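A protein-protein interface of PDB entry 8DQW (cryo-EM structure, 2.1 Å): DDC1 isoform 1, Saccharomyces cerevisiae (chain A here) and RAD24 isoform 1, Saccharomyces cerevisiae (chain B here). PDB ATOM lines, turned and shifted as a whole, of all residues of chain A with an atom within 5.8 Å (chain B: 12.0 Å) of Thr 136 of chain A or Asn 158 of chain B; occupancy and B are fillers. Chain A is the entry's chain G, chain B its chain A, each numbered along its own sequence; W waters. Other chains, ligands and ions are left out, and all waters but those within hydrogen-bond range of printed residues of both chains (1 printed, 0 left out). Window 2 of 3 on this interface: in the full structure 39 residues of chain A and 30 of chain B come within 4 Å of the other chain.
NH1 of Arg 133 of chain A sits at hydrogen-bond distance from O of Ile 156 of chain B (3.1 Å). OG of Ser 58 of chain A is in hydrogen-bond range of ND2 of Asn 158 of chain B (2.8 Å).
No residue of chain B comes within 4 Å of Phe 51 of chain A. No residue of chain B comes within 4 Å of Gly 132 of chain A. Leu 135 of chain A touches none of the printed residues of chain B. Thr 136 of chain A touches one residue of chain B. No residue of chain B comes within 4 Å of Thr 137 of chain A. No residue of chain B comes within 4 Å of Ile 138 of chain A. Ser 139 of chain A touches none of the printed residues of chain B. Arg 140 of chain A touches none of the printed residues of chain B. Asp 154 of chain B touches none of the printed residues of chain A. Of the printed residues of chain A, Ile 156 of chain B touches Arg 133 (3.1 Å). Printed residues of chain A within 4 Å of Val 157 of chain B: Ser 58 and Thr 59. Asn 158 of chain B touches just these residues of chain A: Ser 58, Arg 133 and Thr 136. Printed residues of chain A within 4 Å of Asp 159 of chain B: Tyr 55 (3.7 Å) and Thr 59 (3.7 Å). The nearest residue of chain B that does not touch Thr 136 of chain A is Val 157 of chain B (8.8 Å).
The side-chain hydroxyl (OG1) of Thr 136 of chain A lies within hydrogen-bond range of the backbone carbonyl oxygen (O) of Gly 132 of chain A. The backbone carbonyl oxygen of Tyr 55 of chain A sits at hydrogen-bond distance from the side-chain hydroxyl of Ser 58 of chain A, at 2.6 Å. OD1 of Asn 131 of chain A lies within hydrogen-bond range of N of Arg 133 of chain A (2.9 Å). The side-chain hydroxyl (OG1) of Thr 137 of chain A lies within hydrogen-bond range of the backbone carbonyl oxygen (O) of Arg 133 of chain A.
Among the printed residues, merely in contact across the chains: Tyr 55 of chain A with Asp 159 of chain B (3.7 Å), Ser 58 of chain A with Val 157 of chain B (3.8 Å), Thr 59 of chain A with Val 157 of chain B (3.5 Å), Thr 59 of chain A with Asp 159 of chain B (3.7 Å), Arg 133 of chain A with Asn 158 of chain B (3.6 Å) and Thr 136 of chain A with Asn 158 of chain B (3.7 Å).
Water W1 lies within hydrogen-bond range of O of Arg 133 of chain A (2.7 Å), OG1 of Thr 137 of chain A (3.0 Å) and ND2 of Asn 158 of chain B (3.1 Å).
Of the 14 printed residues of chain B, 4 touch a printed residue of chain A. Printed residues of chain B that touch a printed residue of chain A: Ile 156, Val 157, Asn 158 and Asp 159. Hydrophobic or aromatic side chains of chain B that line the printed part of chain A: Ile 156 and Val 157. Of the 16 printed residues of chain A, 5 touch a printed residue of chain B. Hydrophobic or aromatic side chains of chain A within 4 Å of the printed part of chain B: Tyr 55. Among the printed residues, no Asp or Glu carboxylate lies within 4 Å of a Lys or Arg side-chain nitrogen of the other chain.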
ATOM      1  N   PHE A  51       1.439 -12.625  26.696  1.00  0.00           N
ATOM      2  CA  PHE A  51       1.908 -12.591  25.316  1.00  0.00           C
ATOM      3  C   PHE A  51       2.708 -11.327  25.036  1.00  0.00           C
ATOM      4  O   PHE A  51       3.750 -11.380  24.375  1.00  0.00           O
ATOM      5  CB  PHE A  51       0.732 -12.688  24.345  1.00  0.00           C
ATOM      6  CG  PHE A  51       1.053 -12.187  22.965  1.00  0.00           C
ATOM      7  CD1 PHE A  51       1.786 -12.966  22.086  1.00  0.00           C
ATOM      8  CD2 PHE A  51       0.643 -10.929  22.556  1.00  0.00           C
ATOM      9  CE1 PHE A  51       2.092 -12.507  20.819  1.00  0.00           C
ATOM     10  CE2 PHE A  51       0.948 -10.464  21.291  1.00  0.00           C
ATOM     11  CZ  PHE A  51       1.673 -11.254  20.422  1.00  0.00           C
ATOM     12  N   ILE A  54       6.171 -11.553  26.677  1.00  0.00           N
ATOM     13  CA  ILE A  54       7.033 -12.475  25.945  1.00  0.00           C
ATOM     14  C   ILE A  54       7.489 -11.842  24.636  1.00  0.00           C
ATOM     15  O   ILE A  54       8.657 -11.960  24.249  1.00  0.00           O
ATOM     16  CB  ILE A  54       6.310 -13.817  25.713  1.00  0.00           C
ATOM     17  CG1 ILE A  54       6.605 -14.792  26.855  1.00  0.00           C
ATOM     18  CG2 ILE A  54       6.739 -14.452  24.396  1.00  0.00           C
ATOM     19  CD1 ILE A  54       6.377 -14.226  28.239  1.00  0.00           C
ATOM     20  N   TYR A  55       6.581 -11.156  23.938  1.00  0.00           N
ATOM     21  CA  TYR A  55       6.939 -10.528  22.671  1.00  0.00           C
ATOM     22  C   TYR A  55       8.011  -9.462  22.863  1.00  0.00           C
ATOM     23  O   TYR A  55       8.978  -9.397  22.094  1.00  0.00           O
ATOM     24  CB  TYR A  55       5.693  -9.923  22.021  1.00  0.00           C
ATOM     25  CG  TYR A  55       5.998  -9.040  20.833  1.00  0.00           C
ATOM     26  CD1 TYR A  55       6.205  -9.586  19.575  1.00  0.00           C
ATOM     27  CD2 TYR A  55       6.085  -7.660  20.971  1.00  0.00           C
ATOM     28  CE1 TYR A  55       6.488  -8.784  18.487  1.00  0.00           C
ATOM     29  CE2 TYR A  55       6.367  -6.851  19.888  1.00  0.00           C
ATOM     30  CZ  TYR A  55       6.568  -7.418  18.650  1.00  0.00           C
ATOM     31  OH  TYR A  55       6.849  -6.616  17.567  1.00  0.00           O
ATOM     32  N   SER A  58      11.289 -10.992  23.587  1.00  0.00           N
ATOM     33  CA  SER A  58      11.828 -11.565  22.358  1.00  0.00           C
ATOM     34  C   SER A  58      12.432 -10.485  21.470  1.00  0.00           C
ATOM     35  O   SER A  58      13.430 -10.724  20.782  1.00  0.00           O
ATOM     36  CB  SER A  58      10.733 -12.326  21.612  1.00  0.00           C
ATOM     37  OG  SER A  58       9.950 -11.450  20.820  1.00  0.00           O
ATOM     38  N   THR A  59      11.828  -9.294  21.457  1.00  0.00           N
ATOM     39  CA  THR A  59      12.422  -8.196  20.702  1.00  0.00           C
ATOM     40  C   THR A  59      13.771  -7.795  21.282  1.00  0.00           C
ATOM     41  O   THR A  59      14.670  -7.387  20.537  1.00  0.00           O
ATOM     42  CB  THR A  59      11.494  -6.977  20.672  1.00  0.00           C
ATOM     43  OG1 THR A  59      11.469  -6.353  21.961  1.00  0.00           O
ATOM     44  CG2 THR A  59      10.080  -7.368  20.263  1.00  0.00           C
ATOM     45  N   ILE A  64      15.028 -15.888  25.487  1.00  0.00           N
ATOM     46  CA  ILE A  64      14.524 -15.395  26.762  1.00  0.00           C
ATOM     47  C   ILE A  64      14.952 -16.369  27.848  1.00  0.00           C
ATOM     48  O   ILE A  64      15.136 -17.568  27.597  1.00  0.00           O
ATOM     49  CB  ILE A  64      12.988 -15.229  26.740  1.00  0.00           C
ATOM     50  CG1 ILE A  64      12.566 -14.279  25.616  1.00  0.00           C
ATOM     51  CG2 ILE A  64      12.486 -14.718  28.084  1.00  0.00           C
ATOM     52  CD1 ILE A  64      11.090 -14.372  25.265  1.00  0.00           C
ATOM     53  N   ASN A 131      13.991 -20.197  23.095  1.00  0.00           N
ATOM     54  CA  ASN A 131      13.893 -19.316  21.937  1.00  0.00           C
ATOM     55  C   ASN A 131      12.715 -18.362  22.097  1.00  0.00           C
ATOM     56  O   ASN A 131      11.573 -18.797  22.280  1.00  0.00           O
ATOM     57  CB  ASN A 131      13.741 -20.146  20.663  1.00  0.00           C
ATOM     58  CG  ASN A 131      13.693 -19.292  19.411  1.00  0.00           C
ATOM     59  OD1 ASN A 131      12.726 -18.571  19.173  1.00  0.00           O
ATOM     60  ND2 ASN A 131      14.742 -19.374  18.600  1.00  0.00           N
ATOM     61  N   GLY A 132      12.996 -17.060  22.025  1.00  0.00           N
ATOM     62  CA  GLY A 132      11.953 -16.072  22.247  1.00  0.00           C
ATOM     63  C   GLY A 132      10.887 -16.072  21.167  1.00  0.00           C
ATOM     64  O   GLY A 132       9.693 -15.982  21.464  1.00  0.00           O
ATOM     65  N   ARG A 133      11.301 -16.164  19.901  1.00  0.00           N
ATOM     66  CA  ARG A 133      10.334 -16.127  18.808  1.00  0.00           C
ATOM     67  C   ARG A 133       9.373 -17.307  18.882  1.00  0.00           C
ATOM     68  O   ARG A 133       8.168 -17.154  18.656  1.00  0.00           O
ATOM     69  CB  ARG A 133      11.063 -16.112  17.464  1.00  0.00           C
ATOM     70  CG  ARG A 133      11.803 -14.815  17.180  1.00  0.00           C
ATOM     71  CD  ARG A 133      12.146 -14.670  15.704  1.00  0.00           C
ATOM     72  NE  ARG A 133      12.695 -15.898  15.140  1.00  0.00           N
ATOM     73  CZ  ARG A 133      13.889 -16.393  15.436  1.00  0.00           C
ATOM     74  NH1 ARG A 133      14.695 -15.791  16.296  1.00  0.00           N
ATOM     75  NH2 ARG A 133      14.284 -17.523  14.857  1.00  0.00           N
ATOM     76  N   HIS A 134       9.892 -18.496  19.195  1.00  0.00           N
ATOM     77  CA  HIS A 134       9.041 -19.678  19.278  1.00  0.00           C
ATOM     78  C   HIS A 134       8.003 -19.529  20.384  1.00  0.00           C
ATOM     79  O   HIS A 134       6.819 -19.826  20.188  1.00  0.00           O
ATOM     80  CB  HIS A 134       9.903 -20.919  19.507  1.00  0.00           C
ATOM     81  CG  HIS A 134      10.775 -21.270  18.342  1.00  0.00           C
ATOM     82  ND1 HIS A 134      11.754 -22.237  18.409  1.00  0.00           N
ATOM     83  CD2 HIS A 134      10.818 -20.779  17.081  1.00  0.00           C
ATOM     84  CE1 HIS A 134      12.360 -22.327  17.239  1.00  0.00           C
ATOM     85  NE2 HIS A 134      11.812 -21.453  16.415  1.00  0.00           N
ATOM     86  N   LEU A 135       8.430 -19.059  21.558  1.00  0.00           N
ATOM     87  CA  LEU A 135       7.492 -18.876  22.661  1.00  0.00           C
ATOM     88  C   LEU A 135       6.463 -17.803  22.329  1.00  0.00           C
ATOM     89  O   LEU A 135       5.280 -17.943  22.663  1.00  0.00           O
ATOM     90  CB  LEU A 135       8.248 -18.523  23.943  1.00  0.00           C
ATOM     91  CG  LEU A 135       7.445 -18.599  25.245  1.00  0.00           C
ATOM     92  CD1 LEU A 135       6.809 -19.972  25.429  1.00  0.00           C
ATOM     93  CD2 LEU A 135       8.325 -18.258  26.438  1.00  0.00           C
ATOM     94  N   THR A 136       6.891 -16.722  21.671  1.00  0.00           N
ATOM     95  CA  THR A 136       5.947 -15.681  21.277  1.00  0.00           C
ATOM     96  C   THR A 136       4.903 -16.225  20.311  1.00  0.00           C
ATOM     97  O   THR A 136       3.707 -15.946  20.453  1.00  0.00           O
ATOM     98  CB  THR A 136       6.688 -14.501  20.648  1.00  0.00           C
ATOM     99  OG1 THR A 136       7.680 -14.011  21.560  1.00  0.00           O
ATOM    100  CG2 THR A 136       5.717 -13.377  20.304  1.00  0.00           C
ATOM    101  N   THR A 137       5.336 -17.012  19.324  1.00  0.00           N
ATOM    102  CA  THR A 137       4.384 -17.613  18.394  1.00  0.00           C
ATOM    103  C   THR A 137       3.431 -18.552  19.122  1.00  0.00           C
ATOM    104  O   THR A 137       2.233 -18.591  18.818  1.00  0.00           O
ATOM    105  CB  THR A 137       5.130 -18.358  17.286  1.00  0.00           C
ATOM    106  OG1 THR A 137       5.952 -17.438  16.558  1.00  0.00           O
ATOM    107  CG2 THR A 137       4.149 -19.020  16.328  1.00  0.00           C
ATOM    108  N   ILE A 138       3.942 -19.315  20.089  1.00  0.00           N
ATOM    109  CA  ILE A 138       3.086 -20.232  20.837  1.00  0.00           C
ATOM    110  C   ILE A 138       2.050 -19.462  21.646  1.00  0.00           C
ATOM    111  O   ILE A 138       0.903 -19.904  21.789  1.00  0.00           O
ATOM    112  CB  ILE A 138       3.939 -21.144  21.739  1.00  0.00           C
ATOM    113  CG1 ILE A 138       4.556 -22.279  20.921  1.00  0.00           C
ATOM    114  CG2 ILE A 138       3.098 -21.713  22.876  1.00  0.00           C
ATOM    115  CD1 ILE A 138       5.742 -22.939  21.596  1.00  0.00           C
ATOM    116  N   SER A 139       2.431 -18.309  22.194  1.00  0.00           N
ATOM    117  CA  SER A 139       1.588 -17.589  23.139  1.00  0.00           C
ATOM    118  C   SER A 139       0.592 -16.640  22.482  1.00  0.00           C
ATOM    119  O   SER A 139      -0.247 -16.073  23.187  1.00  0.00           O
ATOM    120  CB  SER A 139       2.462 -16.794  24.116  1.00  0.00           C
ATOM    121  OG  SER A 139       3.477 -17.609  24.676  1.00  0.00           O
ATOM    122  N   ARG A 140       0.655 -16.446  21.167  1.00  0.00           N
ATOM    123  CA  ARG A 140      -0.202 -15.462  20.522  1.00  0.00           C
ATOM    124  C   ARG A 140      -1.630 -15.981  20.393  1.00  0.00           C
ATOM    125  O   ARG A 140      -1.871 -17.181  20.234  1.00  0.00           O
ATOM    126  CB  ARG A 140       0.344 -15.084  19.145  1.00  0.00           C
ATOM    127  CG  ARG A 140       0.613 -16.261  18.225  1.00  0.00           C
ATOM    128  CD  ARG A 140      -0.131 -16.124  16.910  1.00  0.00           C
ATOM    129  NE  ARG A 140      -0.184 -17.388  16.184  1.00  0.00           N
ATOM    130  CZ  ARG A 140      -1.203 -18.236  16.211  1.00  0.00           C
ATOM    131  NH1 ARG A 140      -2.287 -17.997  16.933  1.00  0.00           N
ATOM    132  NH2 ARG A 140      -1.133 -19.356  15.497  1.00  0.00           N
ATOM    133  N   ARG B 152      27.216 -10.435  17.001  1.00  0.00           N
ATOM    134  CA  ARG B 152      26.769 -11.791  16.697  1.00  0.00           C
ATOM    135  C   ARG B 152      25.921 -11.746  15.431  1.00  0.00           C
ATOM    136  O   ARG B 152      24.830 -11.166  15.426  1.00  0.00           O
ATOM    137  CB  ARG B 152      25.987 -12.375  17.871  1.00  0.00           C
ATOM    138  CG  ARG B 152      25.477 -13.786  17.635  1.00  0.00           C
ATOM    139  CD  ARG B 152      25.633 -14.656  18.872  1.00  0.00           C
ATOM    140  NE  ARG B 152      24.627 -14.356  19.882  1.00  0.00           N
ATOM    141  CZ  ARG B 152      23.349 -14.699  19.797  1.00  0.00           C
ATOM    142  NH1 ARG B 152      22.879 -15.364  18.754  1.00  0.00           N
ATOM    143  NH2 ARG B 152      22.521 -14.365  20.783  1.00  0.00           N
ATOM    144  N   ASP B 154      24.430 -14.226  13.720  1.00  0.00           N
ATOM    145  CA  ASP B 154      23.311 -15.155  13.607  1.00  0.00           C
ATOM    146  C   ASP B 154      22.149 -14.805  14.530  1.00  0.00           C
ATOM    147  O   ASP B 154      21.166 -15.550  14.569  1.00  0.00           O
ATOM    148  CB  ASP B 154      23.783 -16.589  13.886  1.00  0.00           C
ATOM    149  CG  ASP B 154      24.137 -16.821  15.345  1.00  0.00           C
ATOM    150  OD1 ASP B 154      24.242 -15.837  16.104  1.00  0.00           O
ATOM    151  OD2 ASP B 154      24.312 -17.997  15.730  1.00  0.00           O
ATOM    152  N   CYS B 155      22.234 -13.699  15.264  1.00  0.00           N
ATOM    153  CA  CYS B 155      21.146 -13.305  16.147  1.00  0.00           C
ATOM    154  C   CYS B 155      19.966 -12.785  15.333  1.00  0.00           C
ATOM    155  O   CYS B 155      20.138 -11.968  14.424  1.00  0.00           O
ATOM    156  CB  CYS B 155      21.622 -12.236  17.129  1.00  0.00           C
ATOM    157  SG  CYS B 155      20.439 -11.847  18.441  1.00  0.00           S
ATOM    158  N   ILE B 156      18.769 -13.267  15.656  1.00  0.00           N
ATOM    159  CA  ILE B 156      17.535 -12.818  15.023  1.00  0.00           C
ATOM    160  C   ILE B 156      16.555 -12.452  16.127  1.00  0.00           C
ATOM    161  O   ILE B 156      16.273 -13.274  17.007  1.00  0.00           O
ATOM    162  CB  ILE B 156      16.934 -13.891  14.100  1.00  0.00           C
ATOM    163  CG1 ILE B 156      17.733 -13.976  12.798  1.00  0.00           C
ATOM    164  CG2 ILE B 156      15.471 -13.579  13.799  1.00  0.00           C
ATOM    165  CD1 ILE B 156      17.503 -15.259  12.024  1.00  0.00           C
ATOM    166  N   VAL B 157      16.038 -11.228  16.080  1.00  0.00           N
ATOM    167  CA  VAL B 157      15.038 -10.764  17.028  1.00  0.00           C
ATOM    168  C   VAL B 157      13.732 -10.524  16.278  1.00  0.00           C
ATOM    169  O   VAL B 157      13.696 -10.442  15.050  1.00  0.00           O
ATOM    170  CB  VAL B 157      15.493  -9.498  17.781  1.00  0.00           C
ATOM    171  CG1 VAL B 157      16.538  -9.852  18.828  1.00  0.00           C
ATOM    172  CG2 VAL B 157      16.035  -8.465  16.807  1.00  0.00           C
ATOM    173  N   ASN B 158      12.645 -10.410  17.041  1.00  0.00           N
ATOM    174  CA  ASN B 158      11.317 -10.375  16.436  1.00  0.00           C
ATOM    175  C   ASN B 158      11.074  -9.071  15.684  1.00  0.00           C
ATOM    176  O   ASN B 158      10.571  -9.081  14.554  1.00  0.00           O
ATOM    177  CB  ASN B 158      10.251 -10.578  17.514  1.00  0.00           C
ATOM    178  CG  ASN B 158       9.468 -11.861  17.326  1.00  0.00           C
ATOM    179  OD1 ASN B 158       9.335 -12.363  16.212  1.00  0.00           O
ATOM    180  ND2 ASN B 158       8.946 -12.401  18.419  1.00  0.00           N
ATOM    181  N   ASP B 159      11.429  -7.938  16.287  1.00  0.00           N
ATOM    182  CA  ASP B 159      11.017  -6.623  15.795  1.00  0.00           C
ATOM    183  C   ASP B 159      12.141  -5.894  15.070  1.00  0.00           C
ATOM    184  O   ASP B 159      12.297  -4.680  15.224  1.00  0.00           O
ATOM    185  CB  ASP B 159      10.492  -5.779  16.953  1.00  0.00           C
ATOM    186  CG  ASP B 159       9.748  -4.542  16.487  1.00  0.00           C
ATOM    187  OD1 ASP B 159       9.458  -4.439  15.276  1.00  0.00           O
ATOM    188  OD2 ASP B 159       9.454  -3.672  17.333  1.00  0.00           O
ATOM    189  N   LEU B 160      12.949  -6.601  14.275  1.00  0.00           N
ATOM    190  CA  LEU B 160      14.042  -5.952  13.568  1.00  0.00           C
ATOM    191  C   LEU B 160      14.358  -6.670  12.261  1.00  0.00           C
ATOM    192  O   LEU B 160      14.619  -7.883  12.286  1.00  0.00           O
ATOM    193  CB  LEU B 160      15.295  -5.902  14.444  1.00  0.00           C
ATOM    194  CG  LEU B 160      15.808  -4.516  14.845  1.00  0.00           C
ATOM    195  CD1 LEU B 160      17.131  -4.638  15.585  1.00  0.00           C
ATOM    196  CD2 LEU B 160      15.959  -3.608  13.633  1.00  0.00           C
ATOM    197  N   PRO B 161      14.347  -5.972  11.123  1.00  0.00           N
ATOM    198  CA  PRO B 161      14.811  -6.599   9.881  1.00  0.00           C
ATOM    199  C   PRO B 161      16.282  -6.975   9.976  1.00  0.00           C
ATOM    200  O   PRO B 161      17.061  -6.351  10.698  1.00  0.00           O
ATOM    201  CB  PRO B 161      14.572  -5.519   8.817  1.00  0.00           C
ATOM    202  CG  PRO B 161      13.589  -4.586   9.417  1.00  0.00           C
ATOM    203  CD  PRO B 161      13.828  -4.614  10.889  1.00  0.00           C
ATOM    204  N   GLN B 162      16.656  -8.019   9.234  1.00  0.00           N
ATOM    205  CA  GLN B 162      18.013  -8.549   9.328  1.00  0.00           C
ATOM    206  C   GLN B 162      19.048  -7.485   8.980  1.00  0.00           C
ATOM    207  O   GLN B 162      20.031  -7.297   9.707  1.00  0.00           O
ATOM    208  CB  GLN B 162      18.162  -9.762   8.411  1.00  0.00           C
ATOM    209  CG  GLN B 162      19.307 -10.685   8.792  1.00  0.00           C
ATOM    210  CD  GLN B 162      18.992 -11.528  10.011  1.00  0.00           C
ATOM    211  OE1 GLN B 162      18.047 -12.314  10.008  1.00  0.00           O
ATOM    212  NE2 GLN B 162      19.783 -11.364  11.065  1.00  0.00           N
ATOM    213  N   MET B 163      18.834  -6.764   7.877  1.00  0.00           N
ATOM    214  CA  MET B 163      19.832  -5.806   7.410  1.00  0.00           C
ATOM    215  C   MET B 163      20.128  -4.726   8.439  1.00  0.00           C
ATOM    216  O   MET B 163      21.212  -4.136   8.406  1.00  0.00           O
ATOM    217  CB  MET B 163      19.373  -5.158   6.104  1.00  0.00           C
ATOM    218  CG  MET B 163      19.233  -6.128   4.944  1.00  0.00           C
ATOM    219  SD  MET B 163      19.415  -5.328   3.339  1.00  0.00           S
ATOM    220  CE  MET B 163      17.838  -4.491   3.193  1.00  0.00           C
ATOM    221  N   GLU B 164      19.195  -4.449   9.349  1.00  0.00           N
ATOM    222  CA  GLU B 164      19.386  -3.415  10.355  1.00  0.00           C
ATOM    223  C   GLU B 164      20.046  -3.927  11.628  1.00  0.00           C
ATOM    224  O   GLU B 164      20.400  -3.114  12.489  1.00  0.00           O
ATOM    225  CB  GLU B 164      18.039  -2.773  10.709  1.00  0.00           C
ATOM    226  CG  GLU B 164      17.144  -2.487   9.510  1.00  0.00           C
ATOM    227  CD  GLU B 164      17.857  -1.721   8.410  1.00  0.00           C
ATOM    228  OE1 GLU B 164      18.824  -0.994   8.716  1.00  0.00           O
ATOM    229  OE2 GLU B 164      17.446  -1.847   7.236  1.00  0.00           O
ATOM    230  N   SER B 165      20.242  -5.241  11.763  1.00  0.00           N
ATOM    231  CA  SER B 165      20.769  -5.783  13.013  1.00  0.00           C
ATOM    232  C   SER B 165      22.068  -5.090  13.406  1.00  0.00           C
ATOM    233  O   SER B 165      22.192  -4.559  14.517  1.00  0.00           O
ATOM    234  CB  SER B 165      20.986  -7.291  12.877  1.00  0.00           C
ATOM    235  OG  SER B 165      21.423  -7.850  14.103  1.00  0.00           O
ATOM    236  N   GLU B 168      21.655  -1.668  14.756  1.00  0.00           N
ATOM    237  CA  GLU B 168      21.255  -1.640  16.158  1.00  0.00           C
ATOM    238  C   GLU B 168      22.460  -1.853  17.067  1.00  0.00           C
ATOM    239  O   GLU B 168      22.658  -1.114  18.039  1.00  0.00           O
ATOM    240  CB  GLU B 168      20.184  -2.699  16.416  1.00  0.00           C
ATOM    241  CG  GLU B 168      19.275  -2.396  17.598  1.00  0.00           C
ATOM    242  CD  GLU B 168      18.371  -1.201  17.355  1.00  0.00           C
ATOM    243  OE1 GLU B 168      18.271  -0.749  16.195  1.00  0.00           O
ATOM    244  OE2 GLU B 168      17.756  -0.715  18.327  1.00  0.00           O
HETATM  245  O   HOH W   1       7.410 -14.889  17.379  1.00  0.00           O
